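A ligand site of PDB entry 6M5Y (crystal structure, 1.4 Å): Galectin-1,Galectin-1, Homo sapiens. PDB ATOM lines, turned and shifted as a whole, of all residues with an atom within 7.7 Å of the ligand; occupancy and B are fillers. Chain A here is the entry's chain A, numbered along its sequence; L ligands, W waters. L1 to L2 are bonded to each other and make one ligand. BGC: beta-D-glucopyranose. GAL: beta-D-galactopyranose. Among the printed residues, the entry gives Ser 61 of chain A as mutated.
Water W5 lies within hydrogen-bond range of O2 of BGC L1 (2.6 Å) and O of His 53 (2.7 Å). Water W8 lies within hydrogen-bond range of an oxygen (O2) of GAL L2 and a ring nitrogen (ND1) of His 53. Water W2 lies within hydrogen-bond range of O4 of GAL L2 and OD1 of Asn 47. Water W3 bridges an oxygen (O6) of GAL L2 (2.8 Å) and the side-chain carboxylate of Glu 72 (3.3 Å).
CE1 of His 53 touches O2 of GAL L2 (3.1 Å). CZ2 of Trp 69 touches C4 of GAL L2, 3.7 Å away. Hydrophobic or aromatic side chains that line the ligand: His 45, His 53 and Trp 69.
The side-chain carboxylate (OE1) of Glu 72 lies within salt-bridge range of the guanidinium group (NH1) of Arg 74 (2.7 Å). The guanidinium group (NE) of Arg 49 lies within hydrogen-bond range of the side-chain amide oxygen (OD1) of Asn 47. The side-chain carboxylate of Asp 55 lies within salt-bridge range of the guanidinium group of Arg 49 (2.7 Å). The backbone carbonyl oxygen (O) of Asn 62 lies within hydrogen-bond range of the backbone NH (N) of His 45, at 2.7 Å. ND2 of Asn 62 is in hydrogen-bond range of O of Gly 70 (2.9 Å). A ring nitrogen (ND1) of His 45 is in hydrogen-bond range of the side-chain amide oxygen of Asn 34, at 2.7 Å. The guanidinium group (NH2) of Arg 74 is in salt-bridge range of the side-chain carboxylate (OD1) of Asp 55 (2.8 Å). O of Val 60 sits at hydrogen-bond distance from N of Asn 47, at 2.8 Å.
OE2 of Glu 72 lies within hydrogen-bond range of O3 of BGC L1. An oxygen (O3) of BGC L1 lies within hydrogen-bond range of the guanidinium group (NH1) of Arg 49 (2.8 Å). The side-chain amide nitrogen of Asn 62 lies within hydrogen-bond range of an oxygen (O6) of GAL L2 (2.8 Å). An oxygen (O4) of GAL L2 lies within hydrogen-bond range of a ring nitrogen (NE2) of His 45 (2.8 Å). NH2 of Arg 74 lies within hydrogen-bond range of O2 of BGC L1. OD1 of Asn 47 lies within hydrogen-bond range of O4 of GAL L2.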
ATOM      1  N   SER A  30     -39.963  23.333  11.440  1.00  0.00           N
ATOM      2  CA  SER A  30     -39.067  24.242  10.760  1.00  0.00           C
ATOM      3  C   SER A  30     -39.880  25.407  10.166  1.00  0.00           C
ATOM      4  O   SER A  30     -41.015  25.204   9.688  1.00  0.00           O
ATOM      5  CB  SER A  30     -38.362  23.452   9.624  1.00  0.00           C
ATOM      6  OG  SER A  30     -37.735  24.294   8.720  1.00  0.00           O
ATOM      7  N   VAL A  32     -39.011  29.161   7.625  1.00  0.00           N
ATOM      8  CA  VAL A  32     -38.071  29.937   6.800  1.00  0.00           C
ATOM      9  C   VAL A  32     -38.626  31.285   6.478  1.00  0.00           C
ATOM     10  O   VAL A  32     -39.792  31.381   6.120  1.00  0.00           O
ATOM     11  CB  VAL A  32     -37.740  29.177   5.503  1.00  0.00           C
ATOM     12  CG1 VAL A  32     -36.850  30.040   4.600  1.00  0.00           C
ATOM     13  CG2 VAL A  32     -37.072  27.848   5.825  1.00  0.00           C
ATOM     14  N   ASN A  34     -37.025  33.861   3.852  1.00  0.00           N
ATOM     15  CA  ASN A  34     -36.049  34.111   2.776  1.00  0.00           C
ATOM     16  C   ASN A  34     -36.113  35.525   2.311  1.00  0.00           C
ATOM     17  O   ASN A  34     -37.125  35.952   1.750  1.00  0.00           O
ATOM     18  CB  ASN A  34     -36.299  33.152   1.604  1.00  0.00           C
ATOM     19  CG  ASN A  34     -35.808  31.747   1.890  1.00  0.00           C
ATOM     20  OD1 ASN A  34     -34.918  31.527   2.719  1.00  0.00           O
ATOM     21  ND2 ASN A  34     -36.416  30.775   1.213  1.00  0.00           N
ATOM     22  N   HIS A  45     -31.311  33.553   4.250  1.00  0.00           N
ATOM     23  CA  HIS A  45     -32.162  32.422   4.507  1.00  0.00           C
ATOM     24  C   HIS A  45     -32.133  32.225   5.987  1.00  0.00           C
ATOM     25  O   HIS A  45     -31.141  31.782   6.521  1.00  0.00           O
ATOM     26  CB  HIS A  45     -31.613  31.197   3.746  1.00  0.00           C
ATOM     27  CG  HIS A  45     -32.212  29.869   4.129  1.00  0.00           C
ATOM     28  ND1 HIS A  45     -33.424  29.453   3.623  1.00  0.00           N
ATOM     29  CD2 HIS A  45     -31.715  28.825   4.835  1.00  0.00           C
ATOM     30  CE1 HIS A  45     -33.676  28.224   4.049  1.00  0.00           C
ATOM     31  NE2 HIS A  45     -32.646  27.820   4.778  1.00  0.00           N
ATOM     32  N   PHE A  46     -33.224  32.640   6.634  1.00  0.00           N
ATOM     33  CA  PHE A  46     -33.334  32.570   8.072  1.00  0.00           C
ATOM     34  C   PHE A  46     -34.215  31.365   8.446  1.00  0.00           C
ATOM     35  O   PHE A  46     -35.400  31.364   8.151  1.00  0.00           O
ATOM     36  CB  PHE A  46     -33.991  33.863   8.599  1.00  0.00           C
ATOM     37  CG  PHE A  46     -34.310  33.828  10.056  1.00  0.00           C
ATOM     38  CD1 PHE A  46     -33.301  33.872  10.991  1.00  0.00           C
ATOM     39  CD2 PHE A  46     -35.611  33.794  10.501  1.00  0.00           C
ATOM     40  CE1 PHE A  46     -33.576  33.848  12.348  1.00  0.00           C
ATOM     41  CE2 PHE A  46     -35.869  33.724  11.850  1.00  0.00           C
ATOM     42  CZ  PHE A  46     -34.868  33.797  12.780  1.00  0.00           C
ATOM     43  N   ASN A  47     -33.603  30.322   9.025  1.00  0.00           N
ATOM     44  CA  ASN A  47     -34.274  29.019   9.196  1.00  0.00           C
ATOM     45  C   ASN A  47     -34.201  28.470  10.643  1.00  0.00           C
ATOM     46  O   ASN A  47     -33.350  27.684  10.960  1.00  0.00           O
ATOM     47  CB  ASN A  47     -33.625  28.063   8.169  1.00  0.00           C
ATOM     48  CG  ASN A  47     -34.208  26.655   8.156  1.00  0.00           C
ATOM     49  OD1 ASN A  47     -33.552  25.745   7.652  1.00  0.00           O
ATOM     50  ND2 ASN A  47     -35.463  26.467   8.653  1.00  0.00           N
ATOM     51  N   ARG A  49     -34.880  25.891  12.987  1.00  0.00           N
ATOM     52  CA  ARG A  49     -35.172  24.465  12.926  1.00  0.00           C
ATOM     53  C   ARG A  49     -35.469  23.921  14.293  1.00  0.00           C
ATOM     54  O   ARG A  49     -34.601  23.822  15.197  1.00  0.00           O
ATOM     55  CB  ARG A  49     -33.998  23.719  12.314  1.00  0.00           C
ATOM     56  CG  ARG A  49     -33.657  24.192  10.922  1.00  0.00           C
ATOM     57  CD  ARG A  49     -32.426  23.463  10.466  1.00  0.00           C
ATOM     58  NE  ARG A  49     -32.093  23.844   9.130  1.00  0.00           N
ATOM     59  CZ  ARG A  49     -30.988  23.478   8.483  1.00  0.00           C
ATOM     60  NH1 ARG A  49     -30.085  22.691   9.066  1.00  0.00           N
ATOM     61  NH2 ARG A  49     -30.797  23.883   7.227  1.00  0.00           N
ATOM     62  N   ALA A  52     -35.355  19.521  12.295  1.00  0.00           N
ATOM     63  CA  ALA A  52     -35.184  19.464  10.856  1.00  0.00           C
ATOM     64  C   ALA A  52     -33.738  19.463  10.498  1.00  0.00           C
ATOM     65  O   ALA A  52     -32.916  20.094  11.179  1.00  0.00           O
ATOM     66  CB  ALA A  52     -35.874  20.629  10.186  1.00  0.00           C
ATOM     67  N   HIS A  53     -33.411  18.751   9.436  1.00  0.00           N
ATOM     68  CA  HIS A  53     -32.107  18.863   8.787  1.00  0.00           C
ATOM     69  C   HIS A  53     -30.942  18.605   9.712  1.00  0.00           C
ATOM     70  O   HIS A  53     -29.874  19.224   9.557  1.00  0.00           O
ATOM     71  CB  HIS A  53     -31.959  20.184   8.046  1.00  0.00           C
ATOM     72  CG  HIS A  53     -32.756  20.270   6.789  1.00  0.00           C
ATOM     73  ND1 HIS A  53     -32.450  19.522   5.661  1.00  0.00           N
ATOM     74  CD2 HIS A  53     -33.808  21.049   6.462  1.00  0.00           C
ATOM     75  CE1 HIS A  53     -33.311  19.807   4.709  1.00  0.00           C
ATOM     76  NE2 HIS A  53     -34.143  20.745   5.156  1.00  0.00           N
ATOM     77  N   GLY A  54     -31.152  17.722  10.674  1.00  0.00           N
ATOM     78  CA  GLY A  54     -30.131  17.300  11.613  1.00  0.00           C
ATOM     79  C   GLY A  54     -29.911  18.245  12.773  1.00  0.00           C
ATOM     80  O   GLY A  54     -28.974  18.081  13.523  1.00  0.00           O
ATOM     81  N   ASP A  55     -30.768  19.252  12.895  1.00  0.00           N
ATOM     82  CA  ASP A  55     -30.687  20.212  14.028  1.00  0.00           C
ATOM     83  C   ASP A  55     -31.929  20.088  14.923  1.00  0.00           C
ATOM     84  O   ASP A  55     -33.039  19.698  14.458  1.00  0.00           O
ATOM     85  CB  ASP A  55     -30.620  21.594  13.462  1.00  0.00           C
ATOM     86  CG  ASP A  55     -29.300  21.894  12.779  1.00  0.00           C
ATOM     87  OD1 ASP A  55     -29.318  22.076  11.552  1.00  0.00           O
ATOM     88  OD2 ASP A  55     -28.235  22.055  13.470  1.00  0.00           O
ATOM     89  N   VAL A  60     -30.487  28.233  11.950  1.00  0.00           N
ATOM     90  CA  VAL A  60     -29.517  28.244  10.809  1.00  0.00           C
ATOM     91  C   VAL A  60     -29.774  29.429   9.830  1.00  0.00           C
ATOM     92  O   VAL A  60     -30.926  29.668   9.380  1.00  0.00           O
ATOM     93  CB  VAL A  60     -29.589  26.911  10.024  1.00  0.00           C
ATOM     94  CG1 VAL A  60     -28.512  26.779   8.949  1.00  0.00           C
ATOM     95  CG2 VAL A  60     -29.536  25.812  10.986  1.00  0.00           C
ATOM     96  N   SER A  61     -28.723  30.183   9.561  1.00  0.00           N
ATOM     97  CA  SER A  61     -28.789  31.227   8.557  1.00  0.00           C
ATOM     98  C   SER A  61     -27.796  30.919   7.456  1.00  0.00           C
ATOM     99  O   SER A  61     -26.747  30.333   7.726  1.00  0.00           O
ATOM    100  CB  SER A  61     -28.508  32.601   9.154  1.00  0.00           C
ATOM    101  OG  SER A  61     -29.448  32.912  10.163  1.00  0.00           O
ATOM    102  N   ASN A  62     -28.170  31.290   6.236  1.00  0.00           N
ATOM    103  CA  ASN A  62     -27.297  31.219   5.063  1.00  0.00           C
ATOM    104  C   ASN A  62     -27.653  32.271   4.051  1.00  0.00           C
ATOM    105  O   ASN A  62     -28.710  32.903   4.138  1.00  0.00           O
ATOM    106  CB  ASN A  62     -27.389  29.807   4.417  1.00  0.00           C
ATOM    107  CG  ASN A  62     -26.069  29.364   3.757  1.00  0.00           C
ATOM    108  OD1 ASN A  62     -25.195  30.169   3.535  1.00  0.00           O
ATOM    109  ND2 ASN A  62     -25.944  28.052   3.480  1.00  0.00           N
ATOM    110  N   SER A  63     -26.739  32.422   3.096  1.00  0.00           N
ATOM    111  CA  SER A  63     -27.005  33.131   1.851  1.00  0.00           C
ATOM    112  C   SER A  63     -27.262  32.107   0.716  1.00  0.00           C
ATOM    113  O   SER A  63     -26.961  30.905   0.862  1.00  0.00           O
ATOM    114  CB  SER A  63     -25.813  33.969   1.494  1.00  0.00           C
ATOM    115  OG  SER A  63     -24.680  33.130   1.310  1.00  0.00           O
ATOM    116  N   LYS A  64     -27.873  32.583  -0.359  1.00  0.00           N
ATOM    117  CA  LYS A  64     -28.089  31.796  -1.563  1.00  0.00           C
ATOM    118  C   LYS A  64     -27.733  32.673  -2.728  1.00  0.00           C
ATOM    119  O   LYS A  64     -28.347  33.699  -2.933  1.00  0.00           O
ATOM    120  CB  LYS A  64     -29.540  31.307  -1.670  1.00  0.00           C
ATOM    121  CG  LYS A  64     -29.710  30.164  -2.685  1.00  0.00           C
ATOM    122  CD  LYS A  64     -31.145  29.652  -2.695  1.00  0.00           C
ATOM    123  CE  LYS A  64     -31.263  28.184  -2.997  1.00  0.00           C
ATOM    124  NZ  LYS A  64     -32.666  27.748  -2.860  1.00  0.00           N
ATOM    125  N   TRP A  69     -26.248  27.630  -2.032  1.00  0.00           N
ATOM    126  CA  TRP A  69     -26.051  27.894  -0.595  1.00  0.00           C
ATOM    127  C   TRP A  69     -24.611  28.205  -0.284  1.00  0.00           C
ATOM    128  O   TRP A  69     -23.711  27.569  -0.838  1.00  0.00           O
ATOM    129  CB  TRP A  69     -26.465  26.676   0.262  1.00  0.00           C
ATOM    130  CG  TRP A  69     -27.895  26.320   0.143  1.00  0.00           C
ATOM    131  CD1 TRP A  69     -28.421  25.175  -0.393  1.00  0.00           C
ATOM    132  CD2 TRP A  69     -29.015  27.138   0.488  1.00  0.00           C
ATOM    133  NE1 TRP A  69     -29.804  25.213  -0.339  1.00  0.00           N
ATOM    134  CE2 TRP A  69     -30.187  26.410   0.179  1.00  0.00           C
ATOM    135  CE3 TRP A  69     -29.141  28.421   1.055  1.00  0.00           C
ATOM    136  CZ2 TRP A  69     -31.468  26.931   0.413  1.00  0.00           C
ATOM    137  CZ3 TRP A  69     -30.434  28.923   1.300  1.00  0.00           C
ATOM    138  CH2 TRP A  69     -31.555  28.193   0.956  1.00  0.00           C
ATOM    139  N   GLY A  70     -24.396  29.126   0.658  1.00  0.00           N
ATOM    140  CA  GLY A  70     -23.059  29.474   1.162  1.00  0.00           C
ATOM    141  C   GLY A  70     -22.712  28.786   2.456  1.00  0.00           C
ATOM    142  O   GLY A  70     -23.178  27.704   2.734  1.00  0.00           O
ATOM    143  N   THR A  71     -21.852  29.427   3.222  1.00  0.00           N
ATOM    144  CA  THR A  71     -21.488  28.953   4.513  1.00  0.00           C
ATOM    145  C   THR A  71     -22.559  29.282   5.574  1.00  0.00           C
ATOM    146  O   THR A  71     -22.964  30.428   5.727  1.00  0.00           O
ATOM    147  CB  THR A  71     -20.121  29.531   4.941  1.00  0.00           C
ATOM    148  OG1 THR A  71     -19.125  29.071   4.027  1.00  0.00           O
ATOM    149  CG2 THR A  71     -19.727  29.111   6.376  1.00  0.00           C
ATOM    150  N   GLU A  72     -22.934  28.262   6.331  1.00  0.00           N
ATOM    151  CA  GLU A  72     -23.970  28.374   7.345  1.00  0.00           C
ATOM    152  C   GLU A  72     -23.465  29.038   8.608  1.00  0.00           C
ATOM    153  O   GLU A  72     -22.265  28.987   8.954  1.00  0.00           O
ATOM    154  CB  GLU A  72     -24.531  27.011   7.705  1.00  0.00           C
ATOM    155  CG  GLU A  72     -25.249  26.354   6.515  1.00  0.00           C
ATOM    156  CD  GLU A  72     -25.771  24.959   6.831  1.00  0.00           C
ATOM    157  OE1 GLU A  72     -25.191  24.260   7.688  1.00  0.00           O
ATOM    158  OE2 GLU A  72     -26.788  24.564   6.233  1.00  0.00           O
ATOM    159  N   GLN A  73     -24.387  29.700   9.280  1.00  0.00           N
ATOM    160  CA  GLN A  73     -24.140  30.278  10.594  1.00  0.00           C
ATOM    161  C   GLN A  73     -25.225  29.754  11.543  1.00  0.00           C
ATOM    162  O   GLN A  73     -26.397  29.913  11.218  1.00  0.00           O
ATOM    163  CB  GLN A  73     -24.188  31.799  10.520  1.00  0.00           C
ATOM    164  CG  GLN A  73     -23.866  32.557  11.788  1.00  0.00           C
ATOM    165  CD  GLN A  73     -23.799  34.066  11.554  1.00  0.00           C
ATOM    166  OE1 GLN A  73     -23.079  34.562  10.638  1.00  0.00           O
ATOM    167  NE2 GLN A  73     -24.586  34.816  12.315  1.00  0.00           N
ATOM    168  N   ARG A  74     -24.849  29.252  12.703  1.00  0.00           N
ATOM    169  CA  ARG A  74     -25.797  28.821  13.684  1.00  0.00           C
ATOM    170  C   ARG A  74     -25.647  29.686  14.940  1.00  0.00           C
ATOM    171  O   ARG A  74     -24.512  29.988  15.354  1.00  0.00           O
ATOM    172  CB  ARG A  74     -25.552  27.366  14.024  1.00  0.00           C
ATOM    173  CG  ARG A  74     -26.043  26.444  12.920  1.00  0.00           C
ATOM    174  CD  ARG A  74     -25.713  25.018  13.213  1.00  0.00           C
ATOM    175  NE  ARG A  74     -26.414  24.069  12.345  1.00  0.00           N
ATOM    176  CZ  ARG A  74     -26.169  23.869  11.057  1.00  0.00           C
ATOM    177  NH1 ARG A  74     -25.193  24.533  10.414  1.00  0.00           N
ATOM    178  NH2 ARG A  74     -26.913  22.961  10.389  1.00  0.00           N
HETATM  179  C2  BGC L   1     -26.250  21.099   6.879  1.00  0.00           C
HETATM  180  C3  BGC L   1     -27.694  21.364   6.534  1.00  0.00           C
HETATM  181  C4  BGC L   1     -27.875  21.396   5.017  1.00  0.00           C
HETATM  182  C5  BGC L   1     -27.324  20.117   4.379  1.00  0.00           C
HETATM  183  C6  BGC L   1     -27.349  20.113   2.899  1.00  0.00           C
HETATM  184  C1  BGC L   1     -25.787  19.825   6.174  1.00  0.00           C
HETATM  185  O1  BGC L   1     -24.402  19.555   6.448  1.00  0.00           O
HETATM  186  O2  BGC L   1     -26.091  20.984   8.257  1.00  0.00           O
HETATM  187  O3  BGC L   1     -28.135  22.599   7.088  1.00  0.00           O
HETATM  188  O4  BGC L   1     -29.273  21.503   4.746  1.00  0.00           O
HETATM  189  O5  BGC L   1     -25.956  19.937   4.768  1.00  0.00           O
HETATM  190  O6  BGC L   1     -26.895  18.822   2.418  1.00  0.00           O
HETATM  191  C1  GAL L   2     -29.662  22.596   3.899  1.00  0.00           C
HETATM  192  C2  GAL L   2     -31.168  22.470   3.596  1.00  0.00           C
HETATM  193  C3  GAL L   2     -31.719  23.727   2.893  1.00  0.00           C
HETATM  194  C4  GAL L   2     -31.289  24.990   3.596  1.00  0.00           C
HETATM  195  C5  GAL L   2     -29.776  24.924   3.821  1.00  0.00           C
HETATM  196  C6  GAL L   2     -29.255  26.192   4.510  1.00  0.00           C
HETATM  197  O2  GAL L   2     -31.387  21.295   2.777  1.00  0.00           O
HETATM  198  O3  GAL L   2     -33.156  23.681   2.830  1.00  0.00           O
HETATM  199  O4  GAL L   2     -31.965  25.065   4.866  1.00  0.00           O
HETATM  200  O5  GAL L   2     -29.406  23.814   4.591  1.00  0.00           O
HETATM  201  O6  GAL L   2     -27.816  26.226   4.490  1.00  0.00           O
HETATM  202  O   HOH W   1     -22.456  21.105   5.601  1.00  0.00           O
HETATM  203  O   HOH W   2     -34.594  24.495   5.342  1.00  0.00           O
HETATM  204  O   HOH W   3     -26.225  24.448   2.987  1.00  0.00           O
HETATM  205  O   HOH W   4     -23.655  21.338   9.239  1.00  0.00           O
HETATM  206  O   HOH W   5     -27.229  19.326   9.958  1.00  0.00           O
HETATM  207  O   HOH W   6     -34.086  21.584   1.575  1.00  0.00           O
HETATM  208  O   HOH W   7     -30.817  21.480   0.080  1.00  0.00           O
HETATM  209  O   HOH W   8     -30.573  18.777   3.090  1.00  0.00           O
HETATM  210  O   HOH W   9     -34.550  25.559   1.777  1.00  0.00           O
HETATM  211  O   HOH W  10     -27.995  17.944   0.367  1.00  0.00           O
